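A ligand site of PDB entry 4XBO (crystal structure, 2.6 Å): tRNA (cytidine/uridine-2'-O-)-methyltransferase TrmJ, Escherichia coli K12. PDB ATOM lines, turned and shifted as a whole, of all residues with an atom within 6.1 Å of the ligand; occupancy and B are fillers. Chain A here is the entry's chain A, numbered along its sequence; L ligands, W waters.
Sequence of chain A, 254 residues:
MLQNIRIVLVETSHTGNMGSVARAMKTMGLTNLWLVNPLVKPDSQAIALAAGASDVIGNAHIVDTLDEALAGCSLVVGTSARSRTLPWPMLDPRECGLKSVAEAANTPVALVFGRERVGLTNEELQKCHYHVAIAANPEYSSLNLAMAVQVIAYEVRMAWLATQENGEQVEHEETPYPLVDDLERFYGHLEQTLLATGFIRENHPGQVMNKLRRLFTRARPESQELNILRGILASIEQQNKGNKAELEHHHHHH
A nitrogen (N4) of the ligand lies within hydrogen-bond range of the backbone carbonyl oxygen (O) of Ile 134, at 3.2 Å.
A nitrogen (N5) of the ligand lies within hydrogen-bond range of the backbone NH (N) of Ile 134.
O of Ser 141 sits at hydrogen-bond distance from N4 of the ligand, 3.0 Å away.
N of Leu 143 lies within hydrogen-bond range of N3 of the ligand, 2.9 Å away.
OG of Ser 80 is in hydrogen-bond range of O2 of the ligand, 3.2 Å away.
The backbone NH (N) of Ala 81 sits at hydrogen-bond distance from an oxygen (O1) of the ligand (2.8 Å).
OG1 of Thr 79 sits at hydrogen-bond distance from O5 of the ligand, at 2.4 Å.
An oxygen (O4) of the ligand sits at hydrogen-bond distance from the backbone NH of Gly 114.
N of Ser 80 is in hydrogen-bond range of O of Val 132.
The backbone carbonyl oxygen (O) of Gly 119 is in hydrogen-bond range of the guanidinium group (NE) of Arg 115, at 3.0 Å.
The side-chain hydroxyl (OG) of Ser 141 lies within hydrogen-bond range of the guanidinium group (NH2) of Arg 82.
The backbone carbonyl oxygen (O) of Val 112 sits at hydrogen-bond distance from the side-chain hydroxyl (OG1) of Thr 79 (2.7 Å).
OG of Ser 80 lies within hydrogen-bond range of O of Arg 82, 3.2 Å away.
Phe 113 touches the ligand.
Arg 115 touches the ligand.
Glu 116 touches the ligand.
Arg 117 touches the ligand.
Gly 119 touches the ligand.
Leu 120 touches the ligand.
O of Val 132 touches C13 of the ligand, 3.2 Å away.
CA of Ala 133 touches N5 of the ligand, at 3.7 Å.
Ser 142 touches the ligand.
CA of Leu 145 touches O3 of the ligand (3.7 Å).
Ala 148 touches the ligand.
Hydrophobic or aromatic side chains within 4 Å of the ligand: Ala 81, Phe 113, Ile 134, Leu 143 and Ala 148.
18 residues have an atom within 4 Å of the ligand: Thr 79, Ser 80, Ala 81, Phe 113, Gly 114, Arg 115, Glu 116, Arg 117, Gly 119, Leu 120, Val 132, Ala 133, Ile 134, Ser 141, Ser 142, Leu 143, Leu 145 and Ala 148.
Along chain A the residues within 4 Å of the ligand span positions 79 to 148.
The nearest printed residue that does not touch the ligand is Val 118 (4.3 Å).
Water W1 lies within hydrogen-bond range of O4 of the ligand (2.5 Å), O of Thr 79 (2.9 Å) and N of Leu 120 (2.9 Å).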
ATOM      1  N   THR A  79     -26.749  31.304 -16.627  1.00  0.00           N
ATOM      2  CA  THR A  79     -26.307  29.942 -16.833  1.00  0.00           C
ATOM      3  C   THR A  79     -25.359  29.845 -18.024  1.00  0.00           C
ATOM      4  O   THR A  79     -25.564  30.488 -19.054  1.00  0.00           O
ATOM      5  CB  THR A  79     -27.496  28.989 -17.083  1.00  0.00           C
ATOM      6  OG1 THR A  79     -28.273  29.494 -18.173  1.00  0.00           O
ATOM      7  CG2 THR A  79     -28.385  28.898 -15.849  1.00  0.00           C
ATOM      8  N   SER A  80     -24.320  29.030 -17.877  1.00  0.00           N
ATOM      9  CA  SER A  80     -23.407  28.777 -18.956  1.00  0.00           C
ATOM     10  C   SER A  80     -22.636  27.490 -18.671  1.00  0.00           C
ATOM     11  O   SER A  80     -22.199  27.263 -17.538  1.00  0.00           O
ATOM     12  CB  SER A  80     -22.453  29.955 -19.127  1.00  0.00           C
ATOM     13  OG  SER A  80     -21.672  29.818 -20.301  1.00  0.00           O
ATOM     14  N   ALA A  81     -22.501  26.635 -19.681  1.00  0.00           N
ATOM     15  CA  ALA A  81     -21.758  25.381 -19.521  1.00  0.00           C
ATOM     16  C   ALA A  81     -20.322  25.637 -19.044  1.00  0.00           C
ATOM     17  O   ALA A  81     -19.756  24.847 -18.275  1.00  0.00           O
ATOM     18  CB  ALA A  81     -21.776  24.571 -20.815  1.00  0.00           C
ATOM     19  N   ARG A  82     -19.734  26.746 -19.503  1.00  0.00           N
ATOM     20  CA  ARG A  82     -18.431  27.193 -19.025  1.00  0.00           C
ATOM     21  C   ARG A  82     -18.209  28.647 -19.411  1.00  0.00           C
ATOM     22  O   ARG A  82     -18.612  29.072 -20.495  1.00  0.00           O
ATOM     23  CB  ARG A  82     -17.317  26.317 -19.601  1.00  0.00           C
ATOM     24  CG  ARG A  82     -17.275  26.259 -21.115  1.00  0.00           C
ATOM     25  CD  ARG A  82     -16.037  25.496 -21.594  1.00  0.00           C
ATOM     26  NE  ARG A  82     -15.980  24.119 -21.077  1.00  0.00           N
ATOM     27  CZ  ARG A  82     -16.317  23.033 -21.778  1.00  0.00           C
ATOM     28  NH1 ARG A  82     -16.734  23.154 -23.032  1.00  0.00           N
ATOM     29  NH2 ARG A  82     -16.226  21.840 -21.225  1.00  0.00           N
ATOM     30  N   VAL A 112     -31.326  33.304 -15.924  1.00  0.00           N
ATOM     31  CA  VAL A 112     -31.220  33.564 -17.357  1.00  0.00           C
ATOM     32  C   VAL A 112     -30.566  32.432 -18.147  1.00  0.00           C
ATOM     33  O   VAL A 112     -29.582  31.835 -17.704  1.00  0.00           O
ATOM     34  CB  VAL A 112     -30.429  34.875 -17.611  1.00  0.00           C
ATOM     35  CG1 VAL A 112     -30.520  35.260 -19.074  1.00  0.00           C
ATOM     36  CG2 VAL A 112     -30.969  36.007 -16.733  1.00  0.00           C
ATOM     37  N   PHE A 113     -31.150  32.147 -19.308  1.00  0.00           N
ATOM     38  CA  PHE A 113     -30.717  31.062 -20.175  1.00  0.00           C
ATOM     39  C   PHE A 113     -30.515  31.605 -21.594  1.00  0.00           C
ATOM     40  O   PHE A 113     -31.132  32.608 -21.987  1.00  0.00           O
ATOM     41  CB  PHE A 113     -31.745  29.912 -20.168  1.00  0.00           C
ATOM     42  CG  PHE A 113     -31.987  29.322 -18.800  1.00  0.00           C
ATOM     43  CD1 PHE A 113     -32.758  29.995 -17.859  1.00  0.00           C
ATOM     44  CD2 PHE A 113     -31.469  28.069 -18.472  1.00  0.00           C
ATOM     45  CE1 PHE A 113     -32.986  29.455 -16.606  1.00  0.00           C
ATOM     46  CE2 PHE A 113     -31.688  27.506 -17.224  1.00  0.00           C
ATOM     47  CZ  PHE A 113     -32.458  28.201 -16.278  1.00  0.00           C
ATOM     48  N   GLY A 114     -29.657  30.937 -22.365  1.00  0.00           N
ATOM     49  CA  GLY A 114     -29.244  31.501 -23.633  1.00  0.00           C
ATOM     50  C   GLY A 114     -29.785  30.852 -24.885  1.00  0.00           C
ATOM     51  O   GLY A 114     -30.604  29.933 -24.823  1.00  0.00           O
ATOM     52  N   ARG A 115     -29.329  31.360 -26.019  1.00  0.00           N
ATOM     53  CA  ARG A 115     -29.648  30.779 -27.307  1.00  0.00           C
ATOM     54  C   ARG A 115     -29.177  29.344 -27.343  1.00  0.00           C
ATOM     55  O   ARG A 115     -28.137  29.025 -26.775  1.00  0.00           O
ATOM     56  CB  ARG A 115     -28.984  31.566 -28.439  1.00  0.00           C
ATOM     57  CG  ARG A 115     -29.588  32.916 -28.707  1.00  0.00           C
ATOM     58  CD  ARG A 115     -28.519  33.885 -29.170  1.00  0.00           C
ATOM     59  NE  ARG A 115     -27.820  34.415 -28.013  1.00  0.00           N
ATOM     60  CZ  ARG A 115     -27.984  35.646 -27.551  1.00  0.00           C
ATOM     61  NH1 ARG A 115     -27.312  36.033 -26.474  1.00  0.00           N
ATOM     62  NH2 ARG A 115     -28.798  36.489 -28.179  1.00  0.00           N
ATOM     63  N   GLU A 116     -29.928  28.485 -28.018  1.00  0.00           N
ATOM     64  CA  GLU A 116     -29.417  27.156 -28.291  1.00  0.00           C
ATOM     65  C   GLU A 116     -28.204  27.314 -29.219  1.00  0.00           C
ATOM     66  O   GLU A 116     -28.119  28.290 -29.967  1.00  0.00           O
ATOM     67  CB  GLU A 116     -30.510  26.256 -28.899  1.00  0.00           C
ATOM     68  CG  GLU A 116     -31.481  26.956 -29.858  1.00  0.00           C
ATOM     69  CD  GLU A 116     -32.713  27.543 -29.170  1.00  0.00           C
ATOM     70  OE1 GLU A 116     -33.624  26.783 -28.790  1.00  0.00           O
ATOM     71  OE2 GLU A 116     -32.788  28.780 -29.028  1.00  0.00           O
ATOM     72  N   ARG A 117     -27.265  26.380 -29.102  1.00  0.00           N
ATOM     73  CA  ARG A 117     -25.994  26.370 -29.846  1.00  0.00           C
ATOM     74  C   ARG A 117     -24.918  27.340 -29.314  1.00  0.00           C
ATOM     75  O   ARG A 117     -23.800  26.921 -29.055  1.00  0.00           O
ATOM     76  CB  ARG A 117     -26.216  26.632 -31.334  1.00  0.00           C
ATOM     77  CG  ARG A 117     -26.710  25.415 -32.111  1.00  0.00           C
ATOM     78  CD  ARG A 117     -25.567  24.481 -32.490  1.00  0.00           C
ATOM     79  NE  ARG A 117     -24.788  24.979 -33.634  1.00  0.00           N
ATOM     80  CZ  ARG A 117     -25.081  24.695 -34.906  1.00  0.00           C
ATOM     81  NH1 ARG A 117     -26.127  23.932 -35.205  1.00  0.00           N
ATOM     82  NH2 ARG A 117     -24.327  25.188 -35.881  1.00  0.00           N
ATOM     83  N   VAL A 118     -25.264  28.620 -29.139  1.00  0.00           N
ATOM     84  CA  VAL A 118     -24.267  29.646 -28.802  1.00  0.00           C
ATOM     85  C   VAL A 118     -24.409  30.242 -27.402  1.00  0.00           C
ATOM     86  O   VAL A 118     -23.523  30.964 -26.937  1.00  0.00           O
ATOM     87  CB  VAL A 118     -24.304  30.791 -29.824  1.00  0.00           C
ATOM     88  CG1 VAL A 118     -23.884  30.298 -31.178  1.00  0.00           C
ATOM     89  CG2 VAL A 118     -25.702  31.396 -29.895  1.00  0.00           C
ATOM     90  N   GLY A 119     -25.510  29.968 -26.737  1.00  0.00           N
ATOM     91  CA  GLY A 119     -25.712  30.433 -25.371  1.00  0.00           C
ATOM     92  C   GLY A 119     -25.863  31.927 -25.227  1.00  0.00           C
ATOM     93  O   GLY A 119     -26.443  32.608 -26.069  1.00  0.00           O
ATOM     94  N   LEU A 120     -25.343  32.444 -24.126  1.00  0.00           N
ATOM     95  CA  LEU A 120     -25.340  33.871 -23.853  1.00  0.00           C
ATOM     96  C   LEU A 120     -24.022  34.525 -24.287  1.00  0.00           C
ATOM     97  O   LEU A 120     -22.948  33.918 -24.191  1.00  0.00           O
ATOM     98  CB  LEU A 120     -25.575  34.111 -22.357  1.00  0.00           C
ATOM     99  CG  LEU A 120     -26.908  33.560 -21.873  1.00  0.00           C
ATOM    100  CD1 LEU A 120     -26.903  33.250 -20.371  1.00  0.00           C
ATOM    101  CD2 LEU A 120     -28.003  34.549 -22.239  1.00  0.00           C
ATOM    102  N   LEU A 125     -23.849  37.763 -20.047  1.00  0.00           N
ATOM    103  CA  LEU A 125     -23.392  37.067 -18.844  1.00  0.00           C
ATOM    104  C   LEU A 125     -22.834  38.033 -17.793  1.00  0.00           C
ATOM    105  O   LEU A 125     -23.043  37.844 -16.599  1.00  0.00           O
ATOM    106  CB  LEU A 125     -22.355  35.988 -19.210  1.00  0.00           C
ATOM    107  CG  LEU A 125     -22.978  34.688 -19.745  1.00  0.00           C
ATOM    108  CD1 LEU A 125     -21.945  33.855 -20.500  1.00  0.00           C
ATOM    109  CD2 LEU A 125     -23.604  33.899 -18.595  1.00  0.00           C
ATOM    110  N   VAL A 132     -23.978  30.002 -13.185  1.00  0.00           N
ATOM    111  CA  VAL A 132     -24.152  28.621 -12.807  1.00  0.00           C
ATOM    112  C   VAL A 132     -23.757  27.719 -13.964  1.00  0.00           C
ATOM    113  O   VAL A 132     -24.278  27.828 -15.083  1.00  0.00           O
ATOM    114  CB  VAL A 132     -25.619  28.301 -12.395  1.00  0.00           C
ATOM    115  CG1 VAL A 132     -25.807  26.791 -12.231  1.00  0.00           C
ATOM    116  CG2 VAL A 132     -25.980  29.027 -11.119  1.00  0.00           C
ATOM    117  N   ALA A 133     -22.817  26.835 -13.679  1.00  0.00           N
ATOM    118  CA  ALA A 133     -22.507  25.781 -14.608  1.00  0.00           C
ATOM    119  C   ALA A 133     -23.014  24.486 -14.005  1.00  0.00           C
ATOM    120  O   ALA A 133     -22.648  24.129 -12.891  1.00  0.00           O
ATOM    121  CB  ALA A 133     -21.030  25.716 -14.864  1.00  0.00           C
ATOM    122  N   ILE A 134     -23.895  23.808 -14.728  1.00  0.00           N
ATOM    123  CA  ILE A 134     -24.258  22.460 -14.338  1.00  0.00           C
ATOM    124  C   ILE A 134     -23.071  21.548 -14.622  1.00  0.00           C
ATOM    125  O   ILE A 134     -22.665  21.406 -15.768  1.00  0.00           O
ATOM    126  CB  ILE A 134     -25.482  21.957 -15.097  1.00  0.00           C
ATOM    127  CG1 ILE A 134     -26.655  22.914 -14.921  1.00  0.00           C
ATOM    128  CG2 ILE A 134     -25.835  20.554 -14.647  1.00  0.00           C
ATOM    129  CD1 ILE A 134     -27.729  22.759 -15.993  1.00  0.00           C
ATOM    130  N   ALA A 135     -22.488  20.967 -13.579  1.00  0.00           N
ATOM    131  CA  ALA A 135     -21.337  20.084 -13.761  1.00  0.00           C
ATOM    132  C   ALA A 135     -21.676  18.958 -14.730  1.00  0.00           C
ATOM    133  O   ALA A 135     -22.594  18.184 -14.513  1.00  0.00           O
ATOM    134  CB  ALA A 135     -20.869  19.521 -12.422  1.00  0.00           C
ATOM    135  N   ALA A 136     -20.936  18.878 -15.818  1.00  0.00           N
ATOM    136  CA  ALA A 136     -21.233  17.916 -16.849  1.00  0.00           C
ATOM    137  C   ALA A 136     -19.983  17.180 -17.329  1.00  0.00           C
ATOM    138  O   ALA A 136     -18.858  17.539 -16.989  1.00  0.00           O
ATOM    139  CB  ALA A 136     -21.916  18.600 -18.019  1.00  0.00           C
ATOM    140  N   SER A 141     -20.621  18.814 -22.608  1.00  0.00           N
ATOM    141  CA  SER A 141     -21.029  19.520 -21.399  1.00  0.00           C
ATOM    142  C   SER A 141     -22.209  20.488 -21.608  1.00  0.00           C
ATOM    143  O   SER A 141     -22.710  21.065 -20.641  1.00  0.00           O
ATOM    144  CB  SER A 141     -19.837  20.282 -20.805  1.00  0.00           C
ATOM    145  OG  SER A 141     -19.318  21.228 -21.708  1.00  0.00           O
ATOM    146  N   SER A 142     -22.654  20.648 -22.845  1.00  0.00           N
ATOM    147  CA  SER A 142     -23.812  21.490 -23.109  1.00  0.00           C
ATOM    148  C   SER A 142     -25.112  20.697 -23.057  1.00  0.00           C
ATOM    149  O   SER A 142     -25.359  19.810 -23.875  1.00  0.00           O
ATOM    150  CB  SER A 142     -23.701  22.187 -24.472  1.00  0.00           C
ATOM    151  OG  SER A 142     -22.615  23.110 -24.470  1.00  0.00           O
ATOM    152  N   LEU A 143     -25.948  21.030 -22.082  1.00  0.00           N
ATOM    153  CA  LEU A 143     -27.294  20.504 -22.026  1.00  0.00           C
ATOM    154  C   LEU A 143     -28.160  21.184 -23.054  1.00  0.00           C
ATOM    155  O   LEU A 143     -27.897  22.306 -23.476  1.00  0.00           O
ATOM    156  CB  LEU A 143     -27.919  20.671 -20.636  1.00  0.00           C
ATOM    157  CG  LEU A 143     -27.457  19.721 -19.540  1.00  0.00           C
ATOM    158  CD1 LEU A 143     -26.093  20.130 -18.992  1.00  0.00           C
ATOM    159  CD2 LEU A 143     -28.497  19.632 -18.425  1.00  0.00           C
ATOM    160  N   ASN A 144     -29.192  20.472 -23.454  1.00  0.00           N
ATOM    161  CA  ASN A 144     -30.294  21.061 -24.183  1.00  0.00           C
ATOM    162  C   ASN A 144     -30.941  22.139 -23.304  1.00  0.00           C
ATOM    163  O   ASN A 144     -31.094  21.916 -22.104  1.00  0.00           O
ATOM    164  CB  ASN A 144     -31.286  19.977 -24.532  1.00  0.00           C
ATOM    165  CG  ASN A 144     -32.020  20.257 -25.791  1.00  0.00           C
ATOM    166  OD1 ASN A 144     -33.078  20.895 -25.788  1.00  0.00           O
ATOM    167  ND2 ASN A 144     -31.469  19.761 -26.907  1.00  0.00           N
ATOM    168  N   LEU A 145     -31.298  23.279 -23.882  1.00  0.00           N
ATOM    169  CA  LEU A 145     -31.909  24.405 -23.130  1.00  0.00           C
ATOM    170  C   LEU A 145     -32.935  23.984 -22.082  1.00  0.00           C
ATOM    171  O   LEU A 145     -32.839  24.341 -20.900  1.00  0.00           O
ATOM    172  CB  LEU A 145     -32.570  25.387 -24.108  1.00  0.00           C
ATOM    173  CG  LEU A 145     -33.409  26.546 -23.597  1.00  0.00           C
ATOM    174  CD1 LEU A 145     -32.604  27.438 -22.692  1.00  0.00           C
ATOM    175  CD2 LEU A 145     -33.948  27.357 -24.776  1.00  0.00           C
ATOM    176  N   ALA A 146     -33.926  23.223 -22.546  1.00  0.00           N
ATOM    177  CA  ALA A 146     -35.025  22.793 -21.709  1.00  0.00           C
ATOM    178  C   ALA A 146     -34.540  21.906 -20.580  1.00  0.00           C
ATOM    179  O   ALA A 146     -35.091  21.960 -19.483  1.00  0.00           O
ATOM    180  CB  ALA A 146     -36.072  22.085 -22.529  1.00  0.00           C
ATOM    181  N   ALA A 148     -31.517  22.075 -19.177  1.00  0.00           N
ATOM    182  CA  ALA A 148     -30.828  22.937 -18.251  1.00  0.00           C
ATOM    183  C   ALA A 148     -31.834  23.646 -17.345  1.00  0.00           C
ATOM    184  O   ALA A 148     -31.611  23.800 -16.121  1.00  0.00           O
ATOM    185  CB  ALA A 148     -29.953  23.948 -18.995  1.00  0.00           C
ATOM    186  N   ILE A 152     -32.076  23.330 -13.171  1.00  0.00           N
ATOM    187  CA  ILE A 152     -32.142  24.526 -12.345  1.00  0.00           C
ATOM    188  C   ILE A 152     -33.478  24.644 -11.555  1.00  0.00           C
ATOM    189  O   ILE A 152     -33.491  24.941 -10.350  1.00  0.00           O
ATOM    190  CB  ILE A 152     -31.911  25.774 -13.201  1.00  0.00           C
ATOM    191  CG1 ILE A 152     -30.524  25.700 -13.833  1.00  0.00           C
ATOM    192  CG2 ILE A 152     -32.001  27.029 -12.380  1.00  0.00           C
ATOM    193  CD1 ILE A 152     -29.413  25.657 -12.827  1.00  0.00           C
HETATM  194  N1  LIG L   1     -22.178  26.694 -25.121  1.00  0.00           N
HETATM  195  C1  LIG L   1     -23.498  27.094 -24.671  1.00  0.00           C
HETATM  196  C2  LIG L   1     -24.468  25.970 -25.080  1.00  0.00           C
HETATM  197  C3  LIG L   1     -25.864  26.433 -25.456  1.00  0.00           C
HETATM  198  S1  LIG L   1     -27.154  25.444 -24.669  1.00  0.00           S
HETATM  199  C4  LIG L   1     -23.523  27.526 -23.169  1.00  0.00           C
HETATM  200  O1  LIG L   1     -23.727  26.756 -22.228  1.00  0.00           O
HETATM  201  O2  LIG L   1     -23.339  28.696 -22.839  1.00  0.00           O
HETATM  202  C5  LIG L   1     -28.361  26.780 -24.508  1.00  0.00           C
HETATM  203  C6  LIG L   1     -28.537  27.252 -23.077  1.00  0.00           C
HETATM  204  O3  LIG L   1     -28.727  26.151 -22.188  1.00  0.00           O
HETATM  205  C7  LIG L   1     -27.311  27.986 -22.556  1.00  0.00           C
HETATM  206  O4  LIG L   1     -27.390  29.355 -22.826  1.00  0.00           O
HETATM  207  C8  LIG L   1     -27.372  27.725 -21.063  1.00  0.00           C
HETATM  208  O5  LIG L   1     -28.246  28.622 -20.440  1.00  0.00           O
HETATM  209  C9  LIG L   1     -28.042  26.380 -20.967  1.00  0.00           C
HETATM  210  N2  LIG L   1     -27.062  25.323 -20.642  1.00  0.00           N
HETATM  211  C10 LIG L   1     -26.719  24.238 -21.389  1.00  0.00           C
HETATM  212  N3  LIG L   1     -25.797  23.531 -20.689  1.00  0.00           N
HETATM  213  C11 LIG L   1     -25.526  24.140 -19.506  1.00  0.00           C
HETATM  214  C12 LIG L   1     -24.666  23.847 -18.442  1.00  0.00           C
HETATM  215  N4  LIG L   1     -23.865  22.758 -18.421  1.00  0.00           N
HETATM  216  N5  LIG L   1     -24.664  24.712 -17.372  1.00  0.00           N
HETATM  217  C13 LIG L   1     -25.466  25.838 -17.346  1.00  0.00           C
HETATM  218  N6  LIG L   1     -26.299  26.116 -18.393  1.00  0.00           N
HETATM  219  C14 LIG L   1     -26.328  25.274 -19.473  1.00  0.00           C
HETATM  220  O   HOH W   1     -25.359  30.516 -21.930  1.00  0.00           O
